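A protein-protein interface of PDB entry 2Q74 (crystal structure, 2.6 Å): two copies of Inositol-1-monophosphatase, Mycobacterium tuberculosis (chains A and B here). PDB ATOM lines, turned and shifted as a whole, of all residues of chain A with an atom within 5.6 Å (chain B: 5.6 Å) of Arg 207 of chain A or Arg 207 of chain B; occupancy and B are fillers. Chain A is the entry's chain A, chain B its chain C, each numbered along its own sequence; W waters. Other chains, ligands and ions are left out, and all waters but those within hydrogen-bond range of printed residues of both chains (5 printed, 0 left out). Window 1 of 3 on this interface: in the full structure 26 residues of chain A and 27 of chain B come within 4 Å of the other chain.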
ATOM      1  N   LEU A 177      28.708   4.818  14.737  1.00  0.00           N
ATOM      2  CA  LEU A 177      30.094   4.957  15.107  1.00  0.00           C
ATOM      3  C   LEU A 177      30.254   4.983  16.625  1.00  0.00           C
ATOM      4  O   LEU A 177      29.590   5.754  17.311  1.00  0.00           O
ATOM      5  CB  LEU A 177      30.640   6.247  14.526  1.00  0.00           C
ATOM      6  CG  LEU A 177      32.088   6.583  14.840  1.00  0.00           C
ATOM      7  CD1 LEU A 177      33.060   5.685  14.057  1.00  0.00           C
ATOM      8  CD2 LEU A 177      32.311   8.031  14.526  1.00  0.00           C
ATOM      9  N   GLY A 178      31.178   4.169  17.127  1.00  0.00           N
ATOM     10  CA  GLY A 178      31.568   4.220  18.522  1.00  0.00           C
ATOM     11  C   GLY A 178      32.845   5.020  18.708  1.00  0.00           C
ATOM     12  O   GLY A 178      33.747   5.005  17.870  1.00  0.00           O
ATOM     13  N   THR A 179      32.935   5.744  19.804  1.00  0.00           N
ATOM     14  CA  THR A 179      34.183   6.435  20.139  1.00  0.00           C
ATOM     15  C   THR A 179      34.471   6.405  21.605  1.00  0.00           C
ATOM     16  O   THR A 179      33.633   6.030  22.405  1.00  0.00           O
ATOM     17  CB  THR A 179      34.173   7.906  19.697  1.00  0.00           C
ATOM     18  OG1 THR A 179      32.955   8.538  20.109  1.00  0.00           O
ATOM     19  CG2 THR A 179      34.277   7.970  18.216  1.00  0.00           C
ATOM     20  N   GLY A 180      35.692   6.786  21.933  1.00  0.00           N
ATOM     21  CA  GLY A 180      36.097   6.969  23.306  1.00  0.00           C
ATOM     22  C   GLY A 180      37.096   8.093  23.400  1.00  0.00           C
ATOM     23  O   GLY A 180      37.553   8.630  22.384  1.00  0.00           O
ATOM     24  N   PHE A 181      37.386   8.478  24.637  1.00  0.00           N
ATOM     25  CA  PHE A 181      38.445   9.429  24.940  1.00  0.00           C
ATOM     26  C   PHE A 181      39.613   8.592  25.413  1.00  0.00           C
ATOM     27  O   PHE A 181      39.485   7.825  26.376  1.00  0.00           O
ATOM     28  CB  PHE A 181      37.993  10.417  26.014  1.00  0.00           C
ATOM     29  CG  PHE A 181      36.942  11.396  25.541  1.00  0.00           C
ATOM     30  CD1 PHE A 181      35.813  11.649  26.308  1.00  0.00           C
ATOM     31  CD2 PHE A 181      37.088  12.068  24.333  1.00  0.00           C
ATOM     32  CE1 PHE A 181      34.855  12.551  25.878  1.00  0.00           C
ATOM     33  CE2 PHE A 181      36.134  12.969  23.905  1.00  0.00           C
ATOM     34  CZ  PHE A 181      35.020  13.215  24.683  1.00  0.00           C
ATOM     35  N   LEU A 195      35.102  15.191  16.914  1.00  0.00           N
ATOM     36  CA  LEU A 195      33.922  14.354  16.777  1.00  0.00           C
ATOM     37  C   LEU A 195      32.710  15.134  16.330  1.00  0.00           C
ATOM     38  O   LEU A 195      31.938  14.653  15.513  1.00  0.00           O
ATOM     39  CB  LEU A 195      33.595  13.626  18.087  1.00  0.00           C
ATOM     40  CG  LEU A 195      34.557  12.493  18.461  1.00  0.00           C
ATOM     41  CD1 LEU A 195      34.147  11.784  19.767  1.00  0.00           C
ATOM     42  CD2 LEU A 195      34.689  11.486  17.298  1.00  0.00           C
ATOM     43  N   ASP A 204      24.614   7.838  13.766  1.00  0.00           N
ATOM     44  CA  ASP A 204      24.567   8.216  15.194  1.00  0.00           C
ATOM     45  C   ASP A 204      25.912   7.825  15.836  1.00  0.00           C
ATOM     46  O   ASP A 204      26.774   7.228  15.200  1.00  0.00           O
ATOM     47  CB  ASP A 204      23.400   7.534  15.919  1.00  0.00           C
ATOM     48  CG  ASP A 204      22.932   8.306  17.198  1.00  0.00           C
ATOM     49  OD1 ASP A 204      23.655   9.198  17.681  1.00  0.00           O
ATOM     50  OD2 ASP A 204      21.835   8.008  17.748  1.00  0.00           O
ATOM     51  N   VAL A 205      26.108   8.193  17.087  1.00  0.00           N
ATOM     52  CA  VAL A 205      27.362   7.937  17.786  1.00  0.00           C
ATOM     53  C   VAL A 205      27.066   7.178  19.075  1.00  0.00           C
ATOM     54  O   VAL A 205      26.030   7.389  19.688  1.00  0.00           O
ATOM     55  CB  VAL A 205      28.107   9.296  18.079  1.00  0.00           C
ATOM     56  CG1 VAL A 205      29.407   9.096  18.821  1.00  0.00           C
ATOM     57  CG2 VAL A 205      28.372  10.026  16.788  1.00  0.00           C
ATOM     58  N   ARG A 206      27.976   6.297  19.462  1.00  0.00           N
ATOM     59  CA  ARG A 206      27.897   5.577  20.724  1.00  0.00           C
ATOM     60  C   ARG A 206      29.192   5.790  21.533  1.00  0.00           C
ATOM     61  O   ARG A 206      30.293   5.770  20.963  1.00  0.00           O
ATOM     62  CB  ARG A 206      27.676   4.074  20.464  1.00  0.00           C
ATOM     63  CG  ARG A 206      26.252   3.642  20.013  1.00  0.00           C
ATOM     64  CD  ARG A 206      25.135   3.973  21.055  1.00  0.00           C
ATOM     65  NE  ARG A 206      24.162   4.912  20.478  1.00  0.00           N
ATOM     66  CZ  ARG A 206      22.969   4.580  19.978  1.00  0.00           C
ATOM     67  NH1 ARG A 206      22.543   3.333  20.020  1.00  0.00           N
ATOM     68  NH2 ARG A 206      22.180   5.504  19.461  1.00  0.00           N
ATOM     69  N   ARG A 207      29.055   6.009  22.847  1.00  0.00           N
ATOM     70  CA  ARG A 207      30.209   6.142  23.738  1.00  0.00           C
ATOM     71  C   ARG A 207      29.988   5.301  24.969  1.00  0.00           C
ATOM     72  O   ARG A 207      29.328   5.723  25.930  1.00  0.00           O
ATOM     73  CB  ARG A 207      30.438   7.616  24.075  1.00  0.00           C
ATOM     74  CG  ARG A 207      31.422   7.979  25.239  1.00  0.00           C
ATOM     75  CD  ARG A 207      32.878   7.852  24.845  1.00  0.00           C
ATOM     76  NE  ARG A 207      33.603   9.024  24.285  1.00  0.00           N
ATOM     77  CZ  ARG A 207      33.105  10.111  23.672  1.00  0.00           C
ATOM     78  NH1 ARG A 207      31.804  10.340  23.516  1.00  0.00           N
ATOM     79  NH2 ARG A 207      33.957  11.021  23.209  1.00  0.00           N
ATOM     80  N   ILE A 208      30.611   4.143  24.974  1.00  0.00           N
ATOM     81  CA  ILE A 208      30.295   3.066  25.893  1.00  0.00           C
ATOM     82  C   ILE A 208      31.280   2.887  27.053  1.00  0.00           C
ATOM     83  O   ILE A 208      30.895   2.380  28.096  1.00  0.00           O
ATOM     84  CB  ILE A 208      30.125   1.765  25.085  1.00  0.00           C
ATOM     85  CG1 ILE A 208      28.803   1.832  24.320  1.00  0.00           C
ATOM     86  CG2 ILE A 208      30.178   0.485  25.962  1.00  0.00           C
ATOM     87  CD1 ILE A 208      28.641   0.700  23.342  1.00  0.00           C
ATOM     88  N   GLY A 209      32.523   3.310  26.899  1.00  0.00           N
ATOM     89  CA  GLY A 209      33.520   3.254  27.959  1.00  0.00           C
ATOM     90  C   GLY A 209      34.460   2.054  27.927  1.00  0.00           C
ATOM     91  O   GLY A 209      35.116   1.781  28.959  1.00  0.00           O
ATOM     92  N   LEU B 177      28.796  11.802  32.973  1.00  0.00           N
ATOM     93  CA  LEU B 177      27.657  12.413  32.303  1.00  0.00           C
ATOM     94  C   LEU B 177      27.199  11.587  31.110  1.00  0.00           C
ATOM     95  O   LEU B 177      28.018  11.176  30.291  1.00  0.00           O
ATOM     96  CB  LEU B 177      28.046  13.806  31.838  1.00  0.00           C
ATOM     97  CG  LEU B 177      26.972  14.613  31.096  1.00  0.00           C
ATOM     98  CD1 LEU B 177      25.820  15.053  32.035  1.00  0.00           C
ATOM     99  CD2 LEU B 177      27.623  15.807  30.402  1.00  0.00           C
ATOM    100  N   GLY B 178      25.897  11.360  31.013  1.00  0.00           N
ATOM    101  CA  GLY B 178      25.324  10.723  29.852  1.00  0.00           C
ATOM    102  C   GLY B 178      24.667  11.735  28.930  1.00  0.00           C
ATOM    103  O   GLY B 178      24.064  12.697  29.384  1.00  0.00           O
ATOM    104  N   THR B 179      24.796  11.531  27.623  1.00  0.00           N
ATOM    105  CA  THR B 179      24.104  12.390  26.676  1.00  0.00           C
ATOM    106  C   THR B 179      23.542  11.628  25.518  1.00  0.00           C
ATOM    107  O   THR B 179      23.847  10.463  25.327  1.00  0.00           O
ATOM    108  CB  THR B 179      25.028  13.485  26.100  1.00  0.00           C
ATOM    109  OG1 THR B 179      26.257  12.903  25.646  1.00  0.00           O
ATOM    110  CG2 THR B 179      25.310  14.519  27.146  1.00  0.00           C
ATOM    111  N   GLY B 180      22.702  12.309  24.759  1.00  0.00           N
ATOM    112  CA  GLY B 180      22.203  11.802  23.497  1.00  0.00           C
ATOM    113  C   GLY B 180      21.921  12.967  22.578  1.00  0.00           C
ATOM    114  O   GLY B 180      22.136  14.120  22.939  1.00  0.00           O
ATOM    115  N   PHE B 181      21.433  12.664  21.389  1.00  0.00           N
ATOM    116  CA  PHE B 181      20.869  13.673  20.509  1.00  0.00           C
ATOM    117  C   PHE B 181      19.384  13.377  20.353  1.00  0.00           C
ATOM    118  O   PHE B 181      18.985  12.204  20.182  1.00  0.00           O
ATOM    119  CB  PHE B 181      21.549  13.652  19.144  1.00  0.00           C
ATOM    120  CG  PHE B 181      23.025  13.998  19.180  1.00  0.00           C
ATOM    121  CD1 PHE B 181      23.941  13.234  18.460  1.00  0.00           C
ATOM    122  CD2 PHE B 181      23.498  15.073  19.932  1.00  0.00           C
ATOM    123  CE1 PHE B 181      25.286  13.536  18.483  1.00  0.00           C
ATOM    124  CE2 PHE B 181      24.843  15.383  19.952  1.00  0.00           C
ATOM    125  CZ  PHE B 181      25.741  14.620  19.212  1.00  0.00           C
ATOM    126  N   LEU B 195      28.886  19.876  23.574  1.00  0.00           N
ATOM    127  CA  LEU B 195      29.394  18.835  24.462  1.00  0.00           C
ATOM    128  C   LEU B 195      30.900  18.882  24.596  1.00  0.00           C
ATOM    129  O   LEU B 195      31.437  18.652  25.672  1.00  0.00           O
ATOM    130  CB  LEU B 195      28.956  17.445  23.989  1.00  0.00           C
ATOM    131  CG  LEU B 195      27.466  17.115  24.182  1.00  0.00           C
ATOM    132  CD1 LEU B 195      27.187  15.654  23.771  1.00  0.00           C
ATOM    133  CD2 LEU B 195      26.977  17.388  25.607  1.00  0.00           C
ATOM    134  N   ASP B 204      33.982  11.880  32.712  1.00  0.00           N
ATOM    135  CA  ASP B 204      33.929  11.230  31.405  1.00  0.00           C
ATOM    136  C   ASP B 204      32.501  11.357  30.866  1.00  0.00           C
ATOM    137  O   ASP B 204      31.605  11.864  31.543  1.00  0.00           O
ATOM    138  CB  ASP B 204      34.328   9.753  31.526  1.00  0.00           C
ATOM    139  CG  ASP B 204      34.850   9.149  30.217  1.00  0.00           C
ATOM    140  OD1 ASP B 204      34.690   9.738  29.117  1.00  0.00           O
ATOM    141  OD2 ASP B 204      35.418   8.043  30.301  1.00  0.00           O
ATOM    142  N   VAL B 205      32.291  10.895  29.647  1.00  0.00           N
ATOM    143  CA  VAL B 205      30.985  10.976  28.992  1.00  0.00           C
ATOM    144  C   VAL B 205      30.511   9.578  28.527  1.00  0.00           C
ATOM    145  O   VAL B 205      31.320   8.720  28.138  1.00  0.00           O
ATOM    146  CB  VAL B 205      31.061  11.963  27.781  1.00  0.00           C
ATOM    147  CG1 VAL B 205      29.733  12.097  27.088  1.00  0.00           C
ATOM    148  CG2 VAL B 205      31.531  13.325  28.238  1.00  0.00           C
ATOM    149  N   ARG B 206      29.205   9.347  28.598  1.00  0.00           N
ATOM    150  CA  ARG B 206      28.609   8.110  28.098  1.00  0.00           C
ATOM    151  C   ARG B 206      27.515   8.477  27.068  1.00  0.00           C
ATOM    152  O   ARG B 206      26.730   9.423  27.303  1.00  0.00           O
ATOM    153  CB  ARG B 206      28.005   7.276  29.251  1.00  0.00           C
ATOM    154  CG  ARG B 206      29.014   6.511  30.150  1.00  0.00           C
ATOM    155  CD  ARG B 206      29.912   5.462  29.383  1.00  0.00           C
ATOM    156  NE  ARG B 206      31.345   5.831  29.457  1.00  0.00           N
ATOM    157  CZ  ARG B 206      32.235   5.286  30.285  1.00  0.00           C
ATOM    158  NH1 ARG B 206      31.895   4.306  31.081  1.00  0.00           N
ATOM    159  NH2 ARG B 206      33.481   5.680  30.294  1.00  0.00           N
ATOM    160  N   ARG B 207      27.472   7.736  25.953  1.00  0.00           N
ATOM    161  CA  ARG B 207      26.421   7.886  24.956  1.00  0.00           C
ATOM    162  C   ARG B 207      25.866   6.511  24.574  1.00  0.00           C
ATOM    163  O   ARG B 207      26.448   5.778  23.765  1.00  0.00           O
ATOM    164  CB  ARG B 207      26.978   8.642  23.753  1.00  0.00           C
ATOM    165  CG  ARG B 207      26.142   8.658  22.439  1.00  0.00           C
ATOM    166  CD  ARG B 207      24.976   9.616  22.502  1.00  0.00           C
ATOM    167  NE  ARG B 207      25.148  11.021  22.047  1.00  0.00           N
ATOM    168  CZ  ARG B 207      26.275  11.746  21.948  1.00  0.00           C
ATOM    169  NH1 ARG B 207      27.486  11.270  22.210  1.00  0.00           N
ATOM    170  NH2 ARG B 207      26.184  13.007  21.556  1.00  0.00           N
ATOM    171  N   ILE B 208      24.707   6.196  25.129  1.00  0.00           N
ATOM    172  CA  ILE B 208      24.186   4.846  25.160  1.00  0.00           C
ATOM    173  C   ILE B 208      23.056   4.556  24.132  1.00  0.00           C
ATOM    174  O   ILE B 208      22.898   3.428  23.642  1.00  0.00           O
ATOM    175  CB  ILE B 208      23.793   4.506  26.623  1.00  0.00           C
ATOM    176  CG1 ILE B 208      25.077   4.286  27.442  1.00  0.00           C
ATOM    177  CG2 ILE B 208      22.882   3.255  26.709  1.00  0.00           C
ATOM    178  CD1 ILE B 208      24.855   4.136  28.942  1.00  0.00           C
ATOM    179  N   GLY B 209      22.306   5.575  23.759  1.00  0.00           N
ATOM    180  CA  GLY B 209      21.253   5.423  22.744  1.00  0.00           C
ATOM    181  C   GLY B 209      19.835   5.268  23.309  1.00  0.00           C
ATOM    182  O   GLY B 209      18.934   4.888  22.595  1.00  0.00           O
HETATM  183  O   HOH W   1      35.095   7.579  26.822  1.00  0.00           O
HETATM  184  O   HOH W   2      34.654   2.703  31.559  1.00  0.00           O
HETATM  185  O   HOH W   3      29.786  12.323  22.794  1.00  0.00           O
HETATM  186  O   HOH W   4      22.603  10.067  20.453  1.00  0.00           O
HETATM  187  O   HOH W   5      19.170   3.646  20.216  1.00  0.00           O
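The backbone carbonyl oxygen (O) of Arg 207 of chain A sits at hydrogen-bond distance from the backbone NH (N) of Arg 207 of chain B (2.7 Å).
The side-chain carboxylate (OD2) of Asp 204 of chain A is in salt-bridge range of the guanidinium group (NH2) of Arg 206 of chain A, at 3.1 Å. NH2 of Arg 206 of chain B is in salt-bridge range of OD2 of Asp 204 of chain B, at 3.1 Å. The backbone NH (N) of Leu 177 of chain B sits at hydrogen-bond distance from the backbone carbonyl oxygen (O) of Asp 204 of chain B. The backbone carbonyl oxygen of Arg 206 of chain B lies within hydrogen-bond range of the backbone NH of Thr 179 of chain B. The backbone carbonyl oxygen (O) of Leu 177 of chain A is in hydrogen-bond range of the backbone NH (N) of Arg 206 of chain A. N of Thr 179 of chain A lies within hydrogen-bond range of O of Arg 206 of chain A (2.9 Å).
Among the printed residues, merely in contact across the chains: Phe 181 of chain A with Asp 204 of chain B, Val 205 of chain A with Arg 207 of chain B, Arg 206 of chain A with Arg 207 of chain B, Arg 206 of chain A with Ile 208 of chain B, Arg 206 of chain A with Gly 209 of chain B, Arg 207 of chain A with Val 205 of chain B, Arg 207 of chain A with Arg 206 of chain B, Ile 208 of chain A with Arg 206 of chain B and Gly 209 of chain A with Arg 206 of chain B.
Of chain B, only Val 205, Arg 206 and Arg 207 come within 4 Å of Arg 207 of chain A. Of chain A, only Val 205 (3.0 Å), Arg 206 (3.4 Å) and Arg 207 (2.7 Å) come within 4 Å of Arg 207 of chain B. Of the printed residues of chain B, Ile 208 of chain A touches Arg 206. Printed residues of chain A within 4 Å of Gly 209 of chain B: Arg 206. Printed residues of chain A within 4 Å of Arg 206 of chain B: Arg 207, Ile 208 and Gly 209. Phe 181 of chain B touches none of the printed residues of chain A. The nearest residue of chain B that does not touch Arg 207 of chain A is Ile 208 of chain B (4.7 Å). The nearest printed residue of chain B that does not touch Ile 208 of chain A is Arg 207 of chain B (4.6 Å).
Printed residues of chain B that touch a printed residue of chain A: Asp 204, Val 205, Arg 206, Arg 207, Ile 208 and Gly 209. Among the printed residues, no Asp or Glu carboxylate lies within 4 Å of a Lys or Arg side-chain nitrogen of the other chain.
Val 205 of chain A touches Arg 207 of chain B, and with the chains exchanged Arg 207 of chain A touches Val 205 of chain B. Arg 206 of chain A touches Arg 207 of chain B, and with the chains exchanged Arg 207 of chain A touches Arg 206 of chain B. Arg 206 of chain A touches Gly 209 of chain B, and with the chains exchanged Gly 209 of chain A touches Arg 206 of chain B. Arg 207 of chain B touches its own counterpart, Arg 207 of chain A. Of the 10 pairs that touch across the chains among the printed residues, 9 have their exchanged pair printed and touching as well.
Water W3 lies within hydrogen-bond range of the guanidinium group (NH1) of Arg 207 of chain B and the guanidinium group (NH1) of Arg 207 of chain A. Water W5 lies within hydrogen-bond range of the backbone carbonyl oxygen of Gly 209 of chain B (2.7 Å) and the guanidinium group of Arg 206 of chain A (3.4 Å). Water W2 bridges O of Gly 209 of chain A and NH1 of Arg 206 of chain B. Water W4 lies within hydrogen-bond range of N of Phe 181 of chain B (3.0 Å), OD1 of Asp 204 of chain A (3.1 Å) and NE of Arg 207 of chain B (3.2 Å). Water W1 lies within hydrogen-bond range of the side-chain carboxylate (OD1) of Asp 204 of chain B (3.2 Å), the guanidinium group (NE) of Arg 207 of chain A (3.3 Å) and the backbone NH (N) of Phe 181 of chain A (3.3 Å).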
